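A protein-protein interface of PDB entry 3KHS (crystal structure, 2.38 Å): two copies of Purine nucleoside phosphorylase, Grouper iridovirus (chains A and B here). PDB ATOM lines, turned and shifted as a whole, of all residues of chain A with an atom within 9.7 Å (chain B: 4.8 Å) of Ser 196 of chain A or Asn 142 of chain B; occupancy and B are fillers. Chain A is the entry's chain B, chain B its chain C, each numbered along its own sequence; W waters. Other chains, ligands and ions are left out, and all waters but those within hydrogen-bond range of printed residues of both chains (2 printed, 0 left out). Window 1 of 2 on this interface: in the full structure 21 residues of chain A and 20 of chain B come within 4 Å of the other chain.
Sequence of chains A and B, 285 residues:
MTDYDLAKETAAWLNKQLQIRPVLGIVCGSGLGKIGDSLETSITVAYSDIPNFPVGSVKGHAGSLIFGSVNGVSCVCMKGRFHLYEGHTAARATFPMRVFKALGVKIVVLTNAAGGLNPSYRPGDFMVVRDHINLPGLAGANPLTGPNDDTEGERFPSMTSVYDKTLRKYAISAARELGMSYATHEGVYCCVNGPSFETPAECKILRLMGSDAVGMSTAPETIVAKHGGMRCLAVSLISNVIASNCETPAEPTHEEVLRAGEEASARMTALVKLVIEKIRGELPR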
ATOM      1  N   LEU A  84     -11.221 -16.273  17.256  1.00  0.00           N
ATOM      2  CA  LEU A  84     -10.531 -14.985  17.183  1.00  0.00           C
ATOM      3  C   LEU A  84      -9.059 -15.084  17.550  1.00  0.00           C
ATOM      4  O   LEU A  84      -8.219 -14.436  16.919  1.00  0.00           O
ATOM      5  CB  LEU A  84     -11.154 -13.951  18.122  1.00  0.00           C
ATOM      6  CG  LEU A  84     -12.161 -13.065  17.418  1.00  0.00           C
ATOM      7  CD1 LEU A  84     -13.326 -13.952  16.981  1.00  0.00           C
ATOM      8  CD2 LEU A  84     -12.660 -11.938  18.363  1.00  0.00           C
ATOM      9  N   TYR A  85      -8.723 -15.894  18.548  1.00  0.00           N
ATOM     10  CA  TYR A  85      -7.323 -15.979  18.970  1.00  0.00           C
ATOM     11  C   TYR A  85      -6.373 -16.575  17.940  1.00  0.00           C
ATOM     12  O   TYR A  85      -5.147 -16.437  18.083  1.00  0.00           O
ATOM     13  CB  TYR A  85      -7.165 -16.721  20.328  1.00  0.00           C
ATOM     14  CG  TYR A  85      -7.500 -18.194  20.297  1.00  0.00           C
ATOM     15  CD1 TYR A  85      -8.671 -18.680  20.905  1.00  0.00           C
ATOM     16  CD2 TYR A  85      -6.679 -19.105  19.629  1.00  0.00           C
ATOM     17  CE1 TYR A  85      -9.017 -20.046  20.849  1.00  0.00           C
ATOM     18  CE2 TYR A  85      -7.012 -20.464  19.563  1.00  0.00           C
ATOM     19  CZ  TYR A  85      -8.190 -20.927  20.185  1.00  0.00           C
ATOM     20  OH  TYR A  85      -8.496 -22.272  20.193  1.00  0.00           O
ATOM     21  N   GLU A  86      -6.899 -17.221  16.899  1.00  0.00           N
ATOM     22  CA  GLU A  86      -5.993 -17.775  15.903  1.00  0.00           C
ATOM     23  C   GLU A  86      -5.576 -16.692  14.936  1.00  0.00           C
ATOM     24  O   GLU A  86      -4.648 -16.877  14.156  1.00  0.00           O
ATOM     25  CB  GLU A  86      -6.639 -18.900  15.104  1.00  0.00           C
ATOM     26  CG  GLU A  86      -7.091 -20.064  15.906  1.00  0.00           C
ATOM     27  CD  GLU A  86      -7.955 -20.969  15.081  1.00  0.00           C
ATOM     28  OE1 GLU A  86      -7.411 -21.621  14.160  1.00  0.00           O
ATOM     29  OE2 GLU A  86      -9.174 -21.019  15.331  1.00  0.00           O
ATOM     30  N   GLY A  87      -6.260 -15.562  14.973  1.00  0.00           N
ATOM     31  CA  GLY A  87      -5.903 -14.488  14.064  1.00  0.00           C
ATOM     32  C   GLY A  87      -7.024 -14.108  13.112  1.00  0.00           C
ATOM     33  O   GLY A  87      -6.905 -13.129  12.382  1.00  0.00           O
ATOM     34  N   PRO A 136     -15.423  -9.258  23.209  1.00  0.00           N
ATOM     35  CA  PRO A 136     -14.836  -8.731  21.969  1.00  0.00           C
ATOM     36  C   PRO A 136     -15.865  -8.020  21.091  1.00  0.00           C
ATOM     37  O   PRO A 136     -15.548  -7.045  20.407  1.00  0.00           O
ATOM     38  CB  PRO A 136     -14.296  -9.970  21.280  1.00  0.00           C
ATOM     39  CG  PRO A 136     -14.017 -10.912  22.398  1.00  0.00           C
ATOM     40  CD  PRO A 136     -15.183 -10.703  23.346  1.00  0.00           C
ATOM     41  N   ALA A 139     -16.532  -4.393  21.947  1.00  0.00           N
ATOM     42  CA  ALA A 139     -15.471  -3.430  21.717  1.00  0.00           C
ATOM     43  C   ALA A 139     -14.535  -3.574  20.540  1.00  0.00           C
ATOM     44  O   ALA A 139     -13.335  -3.714  20.742  1.00  0.00           O
ATOM     45  CB  ALA A 139     -14.636  -3.287  22.999  1.00  0.00           C
ATOM     46  N   ALA A 141     -14.606  -5.965  17.837  1.00  0.00           N
ATOM     47  CA  ALA A 141     -14.443  -7.238  17.156  1.00  0.00           C
ATOM     48  C   ALA A 141     -15.800  -7.950  17.156  1.00  0.00           C
ATOM     49  O   ALA A 141     -15.958  -9.046  17.680  1.00  0.00           O
ATOM     50  CB  ALA A 141     -13.351  -8.082  17.821  1.00  0.00           C
ATOM     51  N   VAL A 192     -14.347 -14.428  25.712  1.00  0.00           N
ATOM     52  CA  VAL A 192     -13.198 -13.504  25.698  1.00  0.00           C
ATOM     53  C   VAL A 192     -12.335 -13.840  24.496  1.00  0.00           C
ATOM     54  O   VAL A 192     -12.467 -14.925  23.908  1.00  0.00           O
ATOM     55  CB  VAL A 192     -12.317 -13.641  26.955  1.00  0.00           C
ATOM     56  CG1 VAL A 192     -13.109 -13.189  28.171  1.00  0.00           C
ATOM     57  CG2 VAL A 192     -11.828 -15.100  27.101  1.00  0.00           C
ATOM     58  N   ASN A 193     -11.434 -12.931  24.144  1.00  0.00           N
ATOM     59  CA  ASN A 193     -10.583 -13.156  22.997  1.00  0.00           C
ATOM     60  C   ASN A 193      -9.628 -14.336  23.090  1.00  0.00           C
ATOM     61  O   ASN A 193      -9.524 -15.138  22.162  1.00  0.00           O
ATOM     62  CB  ASN A 193      -9.765 -11.909  22.680  1.00  0.00           C
ATOM     63  CG  ASN A 193      -9.260 -11.917  21.251  1.00  0.00           C
ATOM     64  OD1 ASN A 193      -9.920 -11.397  20.354  1.00  0.00           O
ATOM     65  ND2 ASN A 193      -8.111 -12.555  21.021  1.00  0.00           N
ATOM     66  N   GLY A 194      -8.940 -14.460  24.219  1.00  0.00           N
ATOM     67  CA  GLY A 194      -7.947 -15.512  24.348  1.00  0.00           C
ATOM     68  C   GLY A 194      -6.676 -15.013  23.613  1.00  0.00           C
ATOM     69  O   GLY A 194      -6.629 -13.854  23.149  1.00  0.00           O
ATOM     70  N   PRO A 195      -5.665 -15.863  23.436  1.00  0.00           N
ATOM     71  CA  PRO A 195      -5.614 -17.259  23.871  1.00  0.00           C
ATOM     72  C   PRO A 195      -5.087 -17.413  25.297  1.00  0.00           C
ATOM     73  O   PRO A 195      -5.090 -18.502  25.840  1.00  0.00           O
ATOM     74  CB  PRO A 195      -4.689 -17.913  22.835  1.00  0.00           C
ATOM     75  CG  PRO A 195      -3.729 -16.840  22.512  1.00  0.00           C
ATOM     76  CD  PRO A 195      -4.618 -15.588  22.428  1.00  0.00           C
ATOM     77  N   SER A 196      -4.610 -16.329  25.901  1.00  0.00           N
ATOM     78  CA  SER A 196      -4.107 -16.413  27.277  1.00  0.00           C
ATOM     79  C   SER A 196      -5.289 -16.469  28.235  1.00  0.00           C
ATOM     80  O   SER A 196      -6.307 -15.800  28.022  1.00  0.00           O
ATOM     81  CB  SER A 196      -3.290 -15.204  27.612  1.00  0.00           C
ATOM     82  OG  SER A 196      -4.091 -14.050  27.376  1.00  0.00           O
ATOM     83  N   PHE A 197      -5.165 -17.276  29.282  1.00  0.00           N
ATOM     84  CA  PHE A 197      -6.223 -17.380  30.266  1.00  0.00           C
ATOM     85  C   PHE A 197      -6.176 -16.096  31.058  1.00  0.00           C
ATOM     86  O   PHE A 197      -5.157 -15.369  31.029  1.00  0.00           O
ATOM     87  CB  PHE A 197      -6.018 -18.605  31.164  1.00  0.00           C
ATOM     88  CG  PHE A 197      -6.298 -19.918  30.457  1.00  0.00           C
ATOM     89  CD1 PHE A 197      -7.520 -20.123  29.798  1.00  0.00           C
ATOM     90  CD2 PHE A 197      -5.360 -20.955  30.465  1.00  0.00           C
ATOM     91  CE1 PHE A 197      -7.805 -21.341  29.160  1.00  0.00           C
ATOM     92  CE2 PHE A 197      -5.635 -22.182  29.827  1.00  0.00           C
ATOM     93  CZ  PHE A 197      -6.860 -22.370  29.175  1.00  0.00           C
ATOM     94  N   GLU A 198      -7.263 -15.781  31.746  1.00  0.00           N
ATOM     95  CA  GLU A 198      -7.301 -14.527  32.475  1.00  0.00           C
ATOM     96  C   GLU A 198      -6.557 -14.500  33.814  1.00  0.00           C
ATOM     97  O   GLU A 198      -6.321 -15.547  34.449  1.00  0.00           O
ATOM     98  CB  GLU A 198      -8.747 -14.059  32.689  1.00  0.00           C
ATOM     99  CG  GLU A 198      -9.799 -15.114  32.902  1.00  0.00           C
ATOM    100  CD  GLU A 198     -10.218 -15.861  31.622  1.00  0.00           C
ATOM    101  OE1 GLU A 198     -10.308 -15.251  30.519  1.00  0.00           O
ATOM    102  OE2 GLU A 198     -10.465 -17.085  31.736  1.00  0.00           O
ATOM    103  N   THR A 199      -6.154 -13.295  34.224  1.00  0.00           N
ATOM    104  CA  THR A 199      -5.483 -13.166  35.500  1.00  0.00           C
ATOM    105  C   THR A 199      -6.539 -13.285  36.582  1.00  0.00           C
ATOM    106  O   THR A 199      -7.740 -13.210  36.302  1.00  0.00           O
ATOM    107  CB  THR A 199      -4.793 -11.829  35.664  1.00  0.00           C
ATOM    108  OG1 THR A 199      -5.750 -10.774  35.536  1.00  0.00           O
ATOM    109  CG2 THR A 199      -3.670 -11.690  34.655  1.00  0.00           C
ATOM    110  N   GLU A 202      -8.731 -10.417  36.594  1.00  0.00           N
ATOM    111  CA  GLU A 202      -9.672 -10.369  35.465  1.00  0.00           C
ATOM    112  C   GLU A 202     -10.835 -11.330  35.731  1.00  0.00           C
ATOM    113  O   GLU A 202     -11.987 -11.031  35.460  1.00  0.00           O
ATOM    114  CB  GLU A 202      -8.962 -10.734  34.160  1.00  0.00           C
ATOM    115  CG  GLU A 202      -8.043  -9.633  33.691  1.00  0.00           C
ATOM    116  CD  GLU A 202      -7.006 -10.080  32.688  1.00  0.00           C
ATOM    117  OE1 GLU A 202      -6.873 -11.298  32.461  1.00  0.00           O
ATOM    118  OE2 GLU A 202      -6.306  -9.199  32.139  1.00  0.00           O
ATOM    119  N   LEU A 206     -14.924 -10.924  35.698  1.00  0.00           N
ATOM    120  CA  LEU A 206     -15.849 -11.780  34.975  1.00  0.00           C
ATOM    121  C   LEU A 206     -16.956 -12.298  35.896  1.00  0.00           C
ATOM    122  O   LEU A 206     -18.095 -12.494  35.454  1.00  0.00           O
ATOM    123  CB  LEU A 206     -15.106 -12.943  34.353  1.00  0.00           C
ATOM    124  CG  LEU A 206     -14.662 -12.763  32.907  1.00  0.00           C
ATOM    125  CD1 LEU A 206     -14.057 -11.391  32.659  1.00  0.00           C
ATOM    126  CD2 LEU A 206     -13.706 -13.885  32.562  1.00  0.00           C
ATOM    127  N   VAL A 214     -16.374 -19.411  31.275  1.00  0.00           N
ATOM    128  CA  VAL A 214     -15.650 -18.560  30.325  1.00  0.00           C
ATOM    129  C   VAL A 214     -14.931 -19.387  29.273  1.00  0.00           C
ATOM    130  O   VAL A 214     -14.306 -20.404  29.577  1.00  0.00           O
ATOM    131  CB  VAL A 214     -14.622 -17.660  31.049  1.00  0.00           C
ATOM    132  CG1 VAL A 214     -13.624 -18.504  31.818  1.00  0.00           C
ATOM    133  CG2 VAL A 214     -13.901 -16.775  30.056  1.00  0.00           C
ATOM    134  N   GLY A 215     -15.057 -18.954  28.024  1.00  0.00           N
ATOM    135  CA  GLY A 215     -14.404 -19.643  26.927  1.00  0.00           C
ATOM    136  C   GLY A 215     -14.026 -18.661  25.816  1.00  0.00           C
ATOM    137  O   GLY A 215     -14.316 -17.478  25.908  1.00  0.00           O
ATOM    138  N   MET A 216     -13.414 -19.135  24.741  1.00  0.00           N
ATOM    139  CA  MET A 216     -12.998 -18.212  23.702  1.00  0.00           C
ATOM    140  C   MET A 216     -13.706 -18.392  22.355  1.00  0.00           C
ATOM    141  O   MET A 216     -13.112 -18.124  21.293  1.00  0.00           O
ATOM    142  CB  MET A 216     -11.479 -18.306  23.535  1.00  0.00           C
ATOM    143  CG  MET A 216     -10.690 -18.116  24.857  1.00  0.00           C
ATOM    144  SD  MET A 216      -9.038 -18.844  24.766  1.00  0.00           S
ATOM    145  CE  MET A 216      -8.429 -18.600  26.436  1.00  0.00           C
ATOM    146  N   ALA B  90      -1.183  -5.438  19.190  1.00  0.00           N
ATOM    147  CA  ALA B  90      -0.695  -5.915  20.459  1.00  0.00           C
ATOM    148  C   ALA B  90       0.537  -6.805  20.233  1.00  0.00           C
ATOM    149  O   ALA B  90       1.523  -6.719  20.987  1.00  0.00           O
ATOM    150  CB  ALA B  90      -1.821  -6.660  21.177  1.00  0.00           C
ATOM    151  N   PRO B 136      -7.740  -4.330  26.740  1.00  0.00           N
ATOM    152  CA  PRO B 136      -7.621  -4.619  25.305  1.00  0.00           C
ATOM    153  C   PRO B 136      -7.477  -6.093  24.991  1.00  0.00           C
ATOM    154  O   PRO B 136      -8.002  -6.580  23.989  1.00  0.00           O
ATOM    155  CB  PRO B 136      -6.384  -3.839  24.888  1.00  0.00           C
ATOM    156  CG  PRO B 136      -6.255  -2.744  25.950  1.00  0.00           C
ATOM    157  CD  PRO B 136      -6.653  -3.450  27.202  1.00  0.00           C
ATOM    158  N   GLY B 137      -6.760  -6.806  25.851  1.00  0.00           N
ATOM    159  CA  GLY B 137      -6.530  -8.226  25.636  1.00  0.00           C
ATOM    160  C   GLY B 137      -7.729  -9.130  25.900  1.00  0.00           C
ATOM    161  O   GLY B 137      -7.685 -10.331  25.589  1.00  0.00           O
ATOM    162  N   GLY B 140     -10.326  -8.327  21.733  1.00  0.00           N
ATOM    163  CA  GLY B 140      -9.902  -7.991  20.388  1.00  0.00           C
ATOM    164  C   GLY B 140      -8.518  -7.434  20.133  1.00  0.00           C
ATOM    165  O   GLY B 140      -8.216  -7.026  19.011  1.00  0.00           O
ATOM    166  N   ALA B 141      -7.682  -7.376  21.157  1.00  0.00           N
ATOM    167  CA  ALA B 141      -6.314  -6.893  20.980  1.00  0.00           C
ATOM    168  C   ALA B 141      -5.424  -7.575  21.999  1.00  0.00           C
ATOM    169  O   ALA B 141      -4.825  -6.940  22.863  1.00  0.00           O
ATOM    170  CB  ALA B 141      -6.238  -5.402  21.116  1.00  0.00           C
ATOM    171  N   ASN B 142      -5.358  -8.892  21.885  1.00  0.00           N
ATOM    172  CA  ASN B 142      -4.549  -9.698  22.766  1.00  0.00           C
ATOM    173  C   ASN B 142      -3.238  -9.918  22.031  1.00  0.00           C
ATOM    174  O   ASN B 142      -3.231 -10.286  20.869  1.00  0.00           O
ATOM    175  CB  ASN B 142      -5.245 -11.005  23.072  1.00  0.00           C
ATOM    176  CG  ASN B 142      -4.471 -11.859  24.052  1.00  0.00           C
ATOM    177  OD1 ASN B 142      -3.408 -12.363  23.732  1.00  0.00           O
ATOM    178  ND2 ASN B 142      -5.010 -12.033  25.252  1.00  0.00           N
ATOM    179  N   PRO B 143      -2.101  -9.698  22.710  1.00  0.00           N
ATOM    180  CA  PRO B 143      -0.793  -9.859  22.067  1.00  0.00           C
ATOM    181  C   PRO B 143      -0.395 -11.269  21.605  1.00  0.00           C
ATOM    182  O   PRO B 143       0.590 -11.427  20.873  1.00  0.00           O
ATOM    183  CB  PRO B 143       0.167  -9.257  23.094  1.00  0.00           C
ATOM    184  CG  PRO B 143      -0.491  -9.641  24.398  1.00  0.00           C
ATOM    185  CD  PRO B 143      -1.954  -9.378  24.139  1.00  0.00           C
ATOM    186  N   LEU B 144      -1.151 -12.282  22.010  1.00  0.00           N
ATOM    187  CA  LEU B 144      -0.829 -13.634  21.598  1.00  0.00           C
ATOM    188  C   LEU B 144      -1.787 -14.058  20.485  1.00  0.00           C
ATOM    189  O   LEU B 144      -1.707 -15.159  19.951  1.00  0.00           O
ATOM    190  CB  LEU B 144      -0.893 -14.578  22.799  1.00  0.00           C
ATOM    191  CG  LEU B 144       0.220 -14.450  23.842  1.00  0.00           C
ATOM    192  CD1 LEU B 144      -0.018 -15.465  24.987  1.00  0.00           C
ATOM    193  CD2 LEU B 144       1.571 -14.725  23.175  1.00  0.00           C
ATOM    194  N   THR B 145      -2.690 -13.165  20.117  1.00  0.00           N
ATOM    195  CA  THR B 145      -3.616 -13.479  19.060  1.00  0.00           C
ATOM    196  C   THR B 145      -2.853 -13.923  17.821  1.00  0.00           C
ATOM    197  O   THR B 145      -1.887 -13.272  17.407  1.00  0.00           O
ATOM    198  CB  THR B 145      -4.402 -12.280  18.725  1.00  0.00           C
ATOM    199  OG1 THR B 145      -5.371 -12.086  19.768  1.00  0.00           O
ATOM    200  CG2 THR B 145      -5.078 -12.464  17.367  1.00  0.00           C
ATOM    201  N   PRO B 157      -1.774 -20.181  27.500  1.00  0.00           N
ATOM    202  CA  PRO B 157      -0.946 -19.978  28.689  1.00  0.00           C
ATOM    203  C   PRO B 157      -1.682 -19.390  29.878  1.00  0.00           C
ATOM    204  O   PRO B 157      -2.508 -18.482  29.740  1.00  0.00           O
ATOM    205  CB  PRO B 157       0.165 -19.068  28.184  1.00  0.00           C
ATOM    206  CG  PRO B 157      -0.539 -18.237  27.137  1.00  0.00           C
ATOM    207  CD  PRO B 157      -1.354 -19.278  26.405  1.00  0.00           C
ATOM    208  N   MET B 159      -2.284 -17.233  33.157  1.00  0.00           N
ATOM    209  CA  MET B 159      -1.889 -15.910  33.603  1.00  0.00           C
ATOM    210  C   MET B 159      -2.243 -15.796  35.076  1.00  0.00           C
ATOM    211  O   MET B 159      -2.483 -14.709  35.587  1.00  0.00           O
ATOM    212  CB  MET B 159      -2.614 -14.817  32.811  1.00  0.00           C
ATOM    213  CG  MET B 159      -2.132 -14.653  31.374  1.00  0.00           C
ATOM    214  SD  MET B 159      -0.387 -14.269  31.217  1.00  0.00           S
ATOM    215  CE  MET B 159       0.180 -15.576  30.062  1.00  0.00           C
ATOM    216  N   ILE B 223       2.246 -10.497  29.481  1.00  0.00           N
ATOM    217  CA  ILE B 223       1.487 -11.660  29.012  1.00  0.00           C
ATOM    218  C   ILE B 223       2.442 -12.459  28.112  1.00  0.00           C
ATOM    219  O   ILE B 223       2.582 -13.668  28.238  1.00  0.00           O
ATOM    220  CB  ILE B 223       0.244 -11.253  28.168  1.00  0.00           C
ATOM    221  CG1 ILE B 223      -0.864 -10.736  29.069  1.00  0.00           C
ATOM    222  CG2 ILE B 223      -0.292 -12.450  27.368  1.00  0.00           C
ATOM    223  CD1 ILE B 223      -2.015 -10.124  28.306  1.00  0.00           C
HETATM  224  O   HOH W   1      -4.787 -17.753  33.960  1.00  0.00           O
HETATM  225  O   HOH W   2      -8.981 -12.575  26.108  1.00  0.00           O
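The backbone NH of Phe 197 of chain A is in hydrogen-bond range of the backbone carbonyl oxygen of Pro 157 of chain B (3.0 Å).
The side-chain amide oxygen of Asn 193 of chain A is in hydrogen-bond range of the backbone NH of Gly 140 of chain B (3.4 Å).
OG1 of Thr 145 of chain B sits at hydrogen-bond distance from ND2 of Asn 193 of chain A (3.0 Å).
OG of Ser 196 of chain A lies within hydrogen-bond range of ND2 of Asn 142 of chain B (3.1 Å).
The side-chain amide nitrogen (ND2) of Asn 142 of chain B lies close to the backbone carbonyl oxygen (O) of Gly 194 of chain A (3.2 Å).
The side-chain amide nitrogen (ND2) of Asn 142 of chain B lies within hydrogen-bond range of the backbone carbonyl oxygen (O) of Gly 137 of chain B (3.2 Å).
OG1 of Thr 145 of chain B is in hydrogen-bond range of O of Asn 142 of chain B, 3.0 Å away.
The backbone NH (N) of Leu 144 of chain B is in hydrogen-bond range of the side-chain amide oxygen (OD1) of Asn 142 of chain B (2.8 Å).
The backbone NH (N) of Thr 199 of chain A is in hydrogen-bond range of the side-chain carboxylate (OE1) of Glu 202 of chain A.
O of Tyr 85 of chain A touches C of Thr 145 of chain B, 3.4 Å away.
CA of Gly 87 of chain A touches CG2 of Thr 145 of chain B, 3.96 Å away.
Asn 193 of chain A touches Gly 137 of chain B (CB to O, 3.9 Å).
Asn 142 of chain B touches Asn 193 of chain A.
CD of Pro 195 of chain A touches OD1 of Asn 142 of chain B (3.7 Å).
Leu 144 of chain B touches Pro 195 of chain A (CB to CG, 3.6 Å).
Pro 157 of chain B touches Pro 195 of chain A (CD to O, 3.9 Å).
Ser 196 of chain A touches Pro 157 of chain B.
Phe 197 of chain A touches Met 159 of chain B.
Met 159 of chain B touches Thr 199 of chain A (O to CA, 3.4 Å).
Printed residues of chain B within 4 Å of Leu 84 of chain A: Thr 145.
Ser 196 of chain A touches just these residues of chain B: Asn 142, Pro 157 and Met 159.
Of chain A, only Asn 193 (3.9 Å) comes within 4 Å of Gly 137 of chain B.
Of chain A, only Asn 193 (3.4 Å) comes within 4 Å of Gly 140 of chain B.
Asn 142 of chain B touches four residues of chain A.
No residue of chain A comes within 4 Å of Pro 143 of chain B.
Of chain A, only Pro 195 comes within 4 Å of Leu 144 of chain B.
Printed residues of chain A within 4 Å of Thr 145 of chain B: Leu 84, Tyr 85, Gly 87, Asn 193 and Pro 195.
Printed residues of chain A within 4 Å of Pro 157 of chain B: Pro 195 (3.9 Å), Ser 196 (3.6 Å) and Phe 197 (3.0 Å).
Of the printed residues of chain A, Met 159 of chain B touches Ser 196, Phe 197 and Thr 199.
The nearest residue of chain B that does not touch Ser 196 of chain A is Ile 223 of chain B (4.1 Å).
The nearest printed residue of chain A that does not touch Asn 142 of chain B is Phe 197 of chain A (6.6 Å).
Printed residues of chain B that touch a printed residue of chain A: Gly 137, Gly 140, Asn 142, Leu 144, Thr 145, Pro 157 and Met 159.
Hydrophobic or aromatic side chains of chain B that line the printed part of chain A: Leu 144, Pro 157 and Met 159.
Among the printed residues, no Asp or Glu carboxylate lies within 4 Å of a Lys or Arg side-chain nitrogen of the other chain.
2 positions are printed for both chains.
Of the 18 pairs that touch across the chains among the printed residues, none has its exchanged pair printed and touching as well.
Water W2 lies within hydrogen-bond range of O of Gly 137 of chain B, N of Gly 194 of chain A and N of Asn 193 of chain A.
Water W1 bridges the backbone NH (N) of Met 159 of chain B (2.7 Å) and the backbone carbonyl oxygen (O) of Glu 198 of chain A (2.7 Å).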
